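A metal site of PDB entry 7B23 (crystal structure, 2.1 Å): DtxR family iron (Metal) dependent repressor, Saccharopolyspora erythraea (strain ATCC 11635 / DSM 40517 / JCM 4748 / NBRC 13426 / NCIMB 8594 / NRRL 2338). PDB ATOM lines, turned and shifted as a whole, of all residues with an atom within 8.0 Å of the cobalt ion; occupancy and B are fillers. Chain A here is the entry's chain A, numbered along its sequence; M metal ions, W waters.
A ring nitrogen (NE2) of His 100 sits at hydrogen-bond distance from OD2 of CSD 104. OE1 of Glu 11 lies within hydrogen-bond range of ND1 of His 108, at 2.6 Å. OD2 of CSD 104 is in salt-bridge range of the guanidinium group (NH1) of Arg 15, at 2.5 Å. A ring nitrogen (ND1) of His 81 sits at hydrogen-bond distance from the side-chain carboxylate (OE1) of Glu 107, at 2.9 Å. The guanidinium group (NH1) of Arg 15 is in salt-bridge range of the side-chain carboxylate (OE1) of Glu 107, at 3.2 Å. The side-chain hydroxyl (OG1) of Thr 16 lies within hydrogen-bond range of the backbone carbonyl oxygen (O) of Met 12 (2.5 Å).
Within 4 Å of the cobalt ion: Met 12, CSD 104, Glu 107 and His 108.
O of CSD 104 is bound to the cobalt ion, at 2.0 Å. The side-chain carboxylate (OE2) of Glu 107 is bound to the cobalt ion (2.0 Å). Water W1 is bound to the cobalt ion, 2.1 Å away. NE2 of His 108 is bound to the cobalt ion (2.2 Å). The cobalt ion is bound by OD1 of CSD 104, at 2.4 Å. The cobalt ion is bound by SD of Met 12, at 2.4 Å. The cobalt ion has six donor atoms within binding distance.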
ATOM      1  N   ASP A   5      13.772  22.918   8.906  1.00  0.00           N
ATOM      2  CA  ASP A   5      14.510  23.127   7.615  1.00  0.00           C
ATOM      3  C   ASP A   5      15.983  22.779   7.817  1.00  0.00           C
ATOM      4  O   ASP A   5      16.436  21.772   7.237  1.00  0.00           O
ATOM      5  CB  ASP A   5      14.295  24.553   7.090  1.00  0.00           C
ATOM      6  CG  ASP A   5      14.663  24.752   5.622  1.00  0.00           C
ATOM      7  OD1 ASP A   5      15.622  24.102   5.166  1.00  0.00           O
ATOM      8  OD2 ASP A   5      13.982  25.559   4.956  1.00  0.00           O
ATOM      9  N   LEU A   6      16.716  23.552   8.634  1.00  0.00           N
ATOM     10  CA  LEU A   6      18.140  23.306   8.966  1.00  0.00           C
ATOM     11  C   LEU A   6      18.253  22.196  10.022  1.00  0.00           C
ATOM     12  O   LEU A   6      19.368  21.655  10.181  1.00  0.00           O
ATOM     13  CB  LEU A   6      18.787  24.606   9.485  1.00  0.00           C
ATOM     14  CG  LEU A   6      18.971  25.722   8.456  1.00  0.00           C
ATOM     15  CD1 LEU A   6      19.622  26.933   9.105  1.00  0.00           C
ATOM     16  CD2 LEU A   6      19.799  25.261   7.261  1.00  0.00           C
ATOM     17  N   ILE A   7      17.158  21.900  10.727  1.00  0.00           N
ATOM     18  CA  ILE A   7      17.069  20.920  11.856  1.00  0.00           C
ATOM     19  C   ILE A   7      17.769  21.527  13.078  1.00  0.00           C
ATOM     20  O   ILE A   7      17.124  21.613  14.130  1.00  0.00           O
ATOM     21  CB  ILE A   7      17.639  19.532  11.478  1.00  0.00           C
ATOM     22  CG1 ILE A   7      17.114  19.034  10.123  1.00  0.00           C
ATOM     23  CG2 ILE A   7      17.373  18.521  12.582  1.00  0.00           C
ATOM     24  CD1 ILE A   7      15.626  18.808  10.075  1.00  0.00           C
ATOM     25  N   ASP A   8      19.042  21.917  12.941  1.00  0.00           N
ATOM     26  CA  ASP A   8      19.866  22.563  14.000  1.00  0.00           C
ATOM     27  C   ASP A   8      20.679  23.704  13.374  1.00  0.00           C
ATOM     28  O   ASP A   8      21.640  23.411  12.654  1.00  0.00           O
ATOM     29  CB  ASP A   8      20.752  21.525  14.695  1.00  0.00           C
ATOM     30  CG  ASP A   8      21.524  22.051  15.895  1.00  0.00           C
ATOM     31  OD1 ASP A   8      21.851  23.249  15.920  1.00  0.00           O
ATOM     32  OD2 ASP A   8      21.804  21.239  16.799  1.00  0.00           O
ATOM     33  N   GLU A  11      24.669  23.892  14.271  1.00  0.00           N
ATOM     34  CA  GLU A  11      25.465  22.820  13.607  1.00  0.00           C
ATOM     35  C   GLU A  11      25.646  23.156  12.125  1.00  0.00           C
ATOM     36  O   GLU A  11      26.737  22.858  11.592  1.00  0.00           O
ATOM     37  CB  GLU A  11      24.809  21.453  13.820  1.00  0.00           C
ATOM     38  CG  GLU A  11      24.939  20.937  15.239  1.00  0.00           C
ATOM     39  CD  GLU A  11      24.433  19.529  15.504  1.00  0.00           C
ATOM     40  OE1 GLU A  11      23.859  18.923  14.574  1.00  0.00           O
ATOM     41  OE2 GLU A  11      24.618  19.044  16.634  1.00  0.00           O
ATOM     42  N   MET A  12      24.647  23.762  11.495  1.00  0.00           N
ATOM     43  CA  MET A  12      24.669  24.075  10.029  1.00  0.00           C
ATOM     44  C   MET A  12      25.532  25.305   9.756  1.00  0.00           C
ATOM     45  O   MET A  12      26.140  25.347   8.674  1.00  0.00           O
ATOM     46  CB  MET A  12      23.249  24.297   9.481  1.00  0.00           C
ATOM     47  CG  MET A  12      22.484  23.004   9.256  1.00  0.00           C
ATOM     48  SD  MET A  12      23.464  21.715   8.444  1.00  0.00           S
ATOM     49  CE  MET A  12      23.896  22.546   6.909  1.00  0.00           C
ATOM     50  N   TYR A  13      25.617  26.264  10.688  1.00  0.00           N
ATOM     51  CA  TYR A  13      26.536  27.420  10.584  1.00  0.00           C
ATOM     52  C   TYR A  13      27.979  26.924  10.723  1.00  0.00           C
ATOM     53  O   TYR A  13      28.830  27.332   9.905  1.00  0.00           O
ATOM     54  CB  TYR A  13      26.209  28.500  11.620  1.00  0.00           C
ATOM     55  CG  TYR A  13      25.186  29.504  11.181  1.00  0.00           C
ATOM     56  CD1 TYR A  13      23.939  29.110  10.721  1.00  0.00           C
ATOM     57  CD2 TYR A  13      25.446  30.866  11.238  1.00  0.00           C
ATOM     58  CE1 TYR A  13      22.986  30.024  10.328  1.00  0.00           C
ATOM     59  CE2 TYR A  13      24.499  31.801  10.848  1.00  0.00           C
ATOM     60  CZ  TYR A  13      23.265  31.379  10.388  1.00  0.00           C
ATOM     61  OH  TYR A  13      22.321  32.290   9.997  1.00  0.00           O
ATOM     62  N   ARG A  15      29.250  23.783  10.257  1.00  0.00           N
ATOM     63  CA  ARG A  15      29.619  22.880   9.133  1.00  0.00           C
ATOM     64  C   ARG A  15      29.752  23.690   7.834  1.00  0.00           C
ATOM     65  O   ARG A  15      30.594  23.312   7.004  1.00  0.00           O
ATOM     66  CB  ARG A  15      28.609  21.738   8.962  1.00  0.00           C
ATOM     67  CG  ARG A  15      29.237  20.430   8.523  1.00  0.00           C
ATOM     68  CD  ARG A  15      28.323  19.643   7.600  1.00  0.00           C
ATOM     69  NE  ARG A  15      28.287  20.222   6.266  1.00  0.00           N
ATOM     70  CZ  ARG A  15      27.300  20.058   5.383  1.00  0.00           C
ATOM     71  NH1 ARG A  15      26.248  19.324   5.688  1.00  0.00           N
ATOM     72  NH2 ARG A  15      27.379  20.633   4.194  1.00  0.00           N
ATOM     73  N   THR A  16      28.965  24.760   7.675  1.00  0.00           N
ATOM     74  CA  THR A  16      29.038  25.675   6.506  1.00  0.00           C
ATOM     75  C   THR A  16      30.383  26.410   6.518  1.00  0.00           C
ATOM     76  O   THR A  16      30.963  26.586   5.428  1.00  0.00           O
ATOM     77  CB  THR A  16      27.865  26.672   6.472  1.00  0.00           C
ATOM     78  OG1 THR A  16      26.656  25.945   6.289  1.00  0.00           O
ATOM     79  CG2 THR A  16      27.989  27.707   5.376  1.00  0.00           C
ATOM     80  N   LEU A  36      23.008  28.975   2.959  1.00  0.00           N
ATOM     81  CA  LEU A  36      21.864  28.537   3.813  1.00  0.00           C
ATOM     82  C   LEU A  36      20.591  29.289   3.410  1.00  0.00           C
ATOM     83  O   LEU A  36      19.520  28.963   3.966  1.00  0.00           O
ATOM     84  CB  LEU A  36      22.205  28.765   5.287  1.00  0.00           C
ATOM     85  CG  LEU A  36      23.397  27.959   5.826  1.00  0.00           C
ATOM     86  CD1 LEU A  36      23.556  28.162   7.315  1.00  0.00           C
ATOM     87  CD2 LEU A  36      23.258  26.482   5.495  1.00  0.00           C
ATOM     88  N   VAL A  77      29.845  16.944  13.617  1.00  0.00           N
ATOM     89  CA  VAL A  77      28.686  17.025  12.658  1.00  0.00           C
ATOM     90  C   VAL A  77      29.118  16.455  11.301  1.00  0.00           C
ATOM     91  O   VAL A  77      28.366  15.645  10.734  1.00  0.00           O
ATOM     92  CB  VAL A  77      28.147  18.462  12.526  1.00  0.00           C
ATOM     93  CG1 VAL A  77      27.092  18.566  11.433  1.00  0.00           C
ATOM     94  CG2 VAL A  77      27.602  18.993  13.841  1.00  0.00           C
ATOM     95  N   HIS A  81      27.823  13.167   9.232  1.00  0.00           N
ATOM     96  CA  HIS A  81      27.389  13.426   7.838  1.00  0.00           C
ATOM     97  C   HIS A  81      27.968  12.368   6.885  1.00  0.00           C
ATOM     98  O   HIS A  81      27.183  11.710   6.173  1.00  0.00           O
ATOM     99  CB  HIS A  81      27.803  14.833   7.411  1.00  0.00           C
ATOM    100  CG  HIS A  81      27.380  15.195   6.033  1.00  0.00           C
ATOM    101  ND1 HIS A  81      26.148  15.758   5.777  1.00  0.00           N
ATOM    102  CD2 HIS A  81      28.007  15.090   4.847  1.00  0.00           C
ATOM    103  CE1 HIS A  81      26.039  15.982   4.480  1.00  0.00           C
ATOM    104  NE2 HIS A  81      27.168  15.580   3.891  1.00  0.00           N
ATOM    105  N   HIS A 100      23.281  13.028  -0.033  1.00  0.00           N
ATOM    106  CA  HIS A 100      23.757  14.212   0.728  1.00  0.00           C
ATOM    107  C   HIS A 100      22.570  14.876   1.441  1.00  0.00           C
ATOM    108  O   HIS A 100      22.686  15.111   2.660  1.00  0.00           O
ATOM    109  CB  HIS A 100      24.472  15.220  -0.181  1.00  0.00           C
ATOM    110  CG  HIS A 100      24.810  16.500   0.507  1.00  0.00           C
ATOM    111  ND1 HIS A 100      25.932  16.644   1.295  1.00  0.00           N
ATOM    112  CD2 HIS A 100      24.162  17.690   0.542  1.00  0.00           C
ATOM    113  CE1 HIS A 100      25.972  17.862   1.775  1.00  0.00           C
ATOM    114  NE2 HIS A 100      24.901  18.532   1.333  1.00  0.00           N
ATOM    115  N   LEU A 101      21.480  15.144   0.723  1.00  0.00           N
ATOM    116  CA  LEU A 101      20.273  15.846   1.239  1.00  0.00           C
ATOM    117  C   LEU A 101      19.745  15.103   2.481  1.00  0.00           C
ATOM    118  O   LEU A 101      19.298  15.786   3.419  1.00  0.00           O
ATOM    119  CB  LEU A 101      19.207  15.916   0.137  1.00  0.00           C
ATOM    120  CG  LEU A 101      17.921  16.663   0.505  1.00  0.00           C
ATOM    121  CD1 LEU A 101      18.218  18.126   0.813  1.00  0.00           C
ATOM    122  CD2 LEU A 101      16.889  16.545  -0.611  1.00  0.00           C
ATOM    123  N   GLU A 102      19.798  13.769   2.464  1.00  0.00           N
ATOM    124  CA  GLU A 102      19.395  12.902   3.596  1.00  0.00           C
ATOM    125  C   GLU A 102      20.388  13.084   4.751  1.00  0.00           C
ATOM    126  O   GLU A 102      19.950  13.345   5.882  1.00  0.00           O
ATOM    127  CB  GLU A 102      19.351  11.438   3.156  1.00  0.00           C
ATOM    128  CG  GLU A 102      18.509  10.557   4.057  1.00  0.00           C
ATOM    129  CD  GLU A 102      16.999  10.765   3.929  1.00  0.00           C
ATOM    130  OE1 GLU A 102      16.558  11.135   2.825  1.00  0.00           O
ATOM    131  OE2 GLU A 102      16.283  10.551   4.922  1.00  0.00           O
ATOM    132  N   ALA A 103      21.689  12.952   4.460  1.00  0.00           N
ATOM    133  CA  ALA A 103      22.813  13.110   5.413  1.00  0.00           C
ATOM    134  C   ALA A 103      22.841  14.524   5.979  1.00  0.00           C
ATOM    135  O   ALA A 103      23.369  14.754   7.071  1.00  0.00           O
ATOM    136  CB  ALA A 103      24.110  12.753   4.725  1.00  0.00           C
ATOM    137  N   CSD A 104      22.277  15.485   5.236  1.00  0.00           N
ATOM    138  CA  CSD A 104      22.173  16.866   5.693  1.00  0.00           C
ATOM    139  CB  CSD A 104      21.639  17.781   4.584  1.00  0.00           C
ATOM    140  SG  CSD A 104      22.615  19.314   4.455  1.00  0.00           S
ATOM    141  C   CSD A 104      21.275  16.951   6.933  1.00  0.00           C
ATOM    142  O   CSD A 104      21.411  17.874   7.731  1.00  0.00           O
ATOM    143  OD1 CSD A 104      22.355  20.065   5.715  1.00  0.00           O
ATOM    144  OD2 CSD A 104      24.162  18.955   4.427  1.00  0.00           O
ATOM    145  N   ARG A 105      20.331  16.017   7.060  1.00  0.00           N
ATOM    146  CA  ARG A 105      19.412  15.991   8.191  1.00  0.00           C
ATOM    147  C   ARG A 105      19.917  14.998   9.244  1.00  0.00           C
ATOM    148  O   ARG A 105      19.910  15.361  10.433  1.00  0.00           O
ATOM    149  CB  ARG A 105      17.999  15.634   7.713  1.00  0.00           C
ATOM    150  CG  ARG A 105      17.371  16.667   6.791  1.00  0.00           C
ATOM    151  CD  ARG A 105      15.868  16.482   6.652  1.00  0.00           C
ATOM    152  NE  ARG A 105      15.529  15.157   6.151  1.00  0.00           N
ATOM    153  CZ  ARG A 105      15.652  14.754   4.884  1.00  0.00           C
ATOM    154  NH1 ARG A 105      16.107  15.586   3.959  1.00  0.00           N
ATOM    155  NH2 ARG A 105      15.319  13.524   4.551  1.00  0.00           N
ATOM    156  N   TRP A 106      20.322  13.796   8.823  1.00  0.00           N
ATOM    157  CA  TRP A 106      20.770  12.680   9.696  1.00  0.00           C
ATOM    158  C   TRP A 106      21.937  13.127  10.584  1.00  0.00           C
ATOM    159  O   TRP A 106      22.033  12.635  11.725  1.00  0.00           O
ATOM    160  CB  TRP A 106      21.154  11.446   8.859  1.00  0.00           C
ATOM    161  CG  TRP A 106      19.990  10.666   8.333  1.00  0.00           C
ATOM    162  CD1 TRP A 106      18.794  11.153   7.882  1.00  0.00           C
ATOM    163  CD2 TRP A 106      19.919   9.244   8.165  1.00  0.00           C
ATOM    164  NE1 TRP A 106      17.982  10.138   7.466  1.00  0.00           N
ATOM    165  CE2 TRP A 106      18.642   8.950   7.634  1.00  0.00           C
ATOM    166  CE3 TRP A 106      20.797   8.177   8.432  1.00  0.00           C
ATOM    167  CZ2 TRP A 106      18.233   7.642   7.349  1.00  0.00           C
ATOM    168  CZ3 TRP A 106      20.395   6.894   8.159  1.00  0.00           C
ATOM    169  CH2 TRP A 106      19.128   6.626   7.619  1.00  0.00           C
ATOM    170  N   GLU A 107      22.797  14.023  10.084  1.00  0.00           N
ATOM    171  CA  GLU A 107      24.041  14.478  10.767  1.00  0.00           C
ATOM    172  C   GLU A 107      23.730  15.126  12.128  1.00  0.00           C
ATOM    173  O   GLU A 107      24.685  15.280  12.918  1.00  0.00           O
ATOM    174  CB  GLU A 107      24.833  15.442   9.886  1.00  0.00           C
ATOM    175  CG  GLU A 107      24.129  16.760   9.592  1.00  0.00           C
ATOM    176  CD  GLU A 107      24.842  17.657   8.596  1.00  0.00           C
ATOM    177  OE1 GLU A 107      25.987  17.339   8.222  1.00  0.00           O
ATOM    178  OE2 GLU A 107      24.258  18.689   8.211  1.00  0.00           O
ATOM    179  N   HIS A 108      22.476  15.480  12.390  1.00  0.00           N
ATOM    180  CA  HIS A 108      22.041  16.251  13.584  1.00  0.00           C
ATOM    181  C   HIS A 108      21.477  15.332  14.678  1.00  0.00           C
ATOM    182  O   HIS A 108      21.438  15.775  15.835  1.00  0.00           O
ATOM    183  CB  HIS A 108      21.062  17.361  13.170  1.00  0.00           C
ATOM    184  CG  HIS A 108      21.599  18.239  12.091  1.00  0.00           C
ATOM    185  ND1 HIS A 108      22.640  19.110  12.300  1.00  0.00           N
ATOM    186  CD2 HIS A 108      21.244  18.366  10.792  1.00  0.00           C
ATOM    187  CE1 HIS A 108      22.921  19.745  11.178  1.00  0.00           C
ATOM    188  NE2 HIS A 108      22.076  19.312  10.241  1.00  0.00           N
HETATM  189 CO    CO M   1      22.410  19.549   8.041  1.00  0.00          CO
HETATM  190  O   HOH W   1      20.621  20.658   7.959  1.00  0.00           O
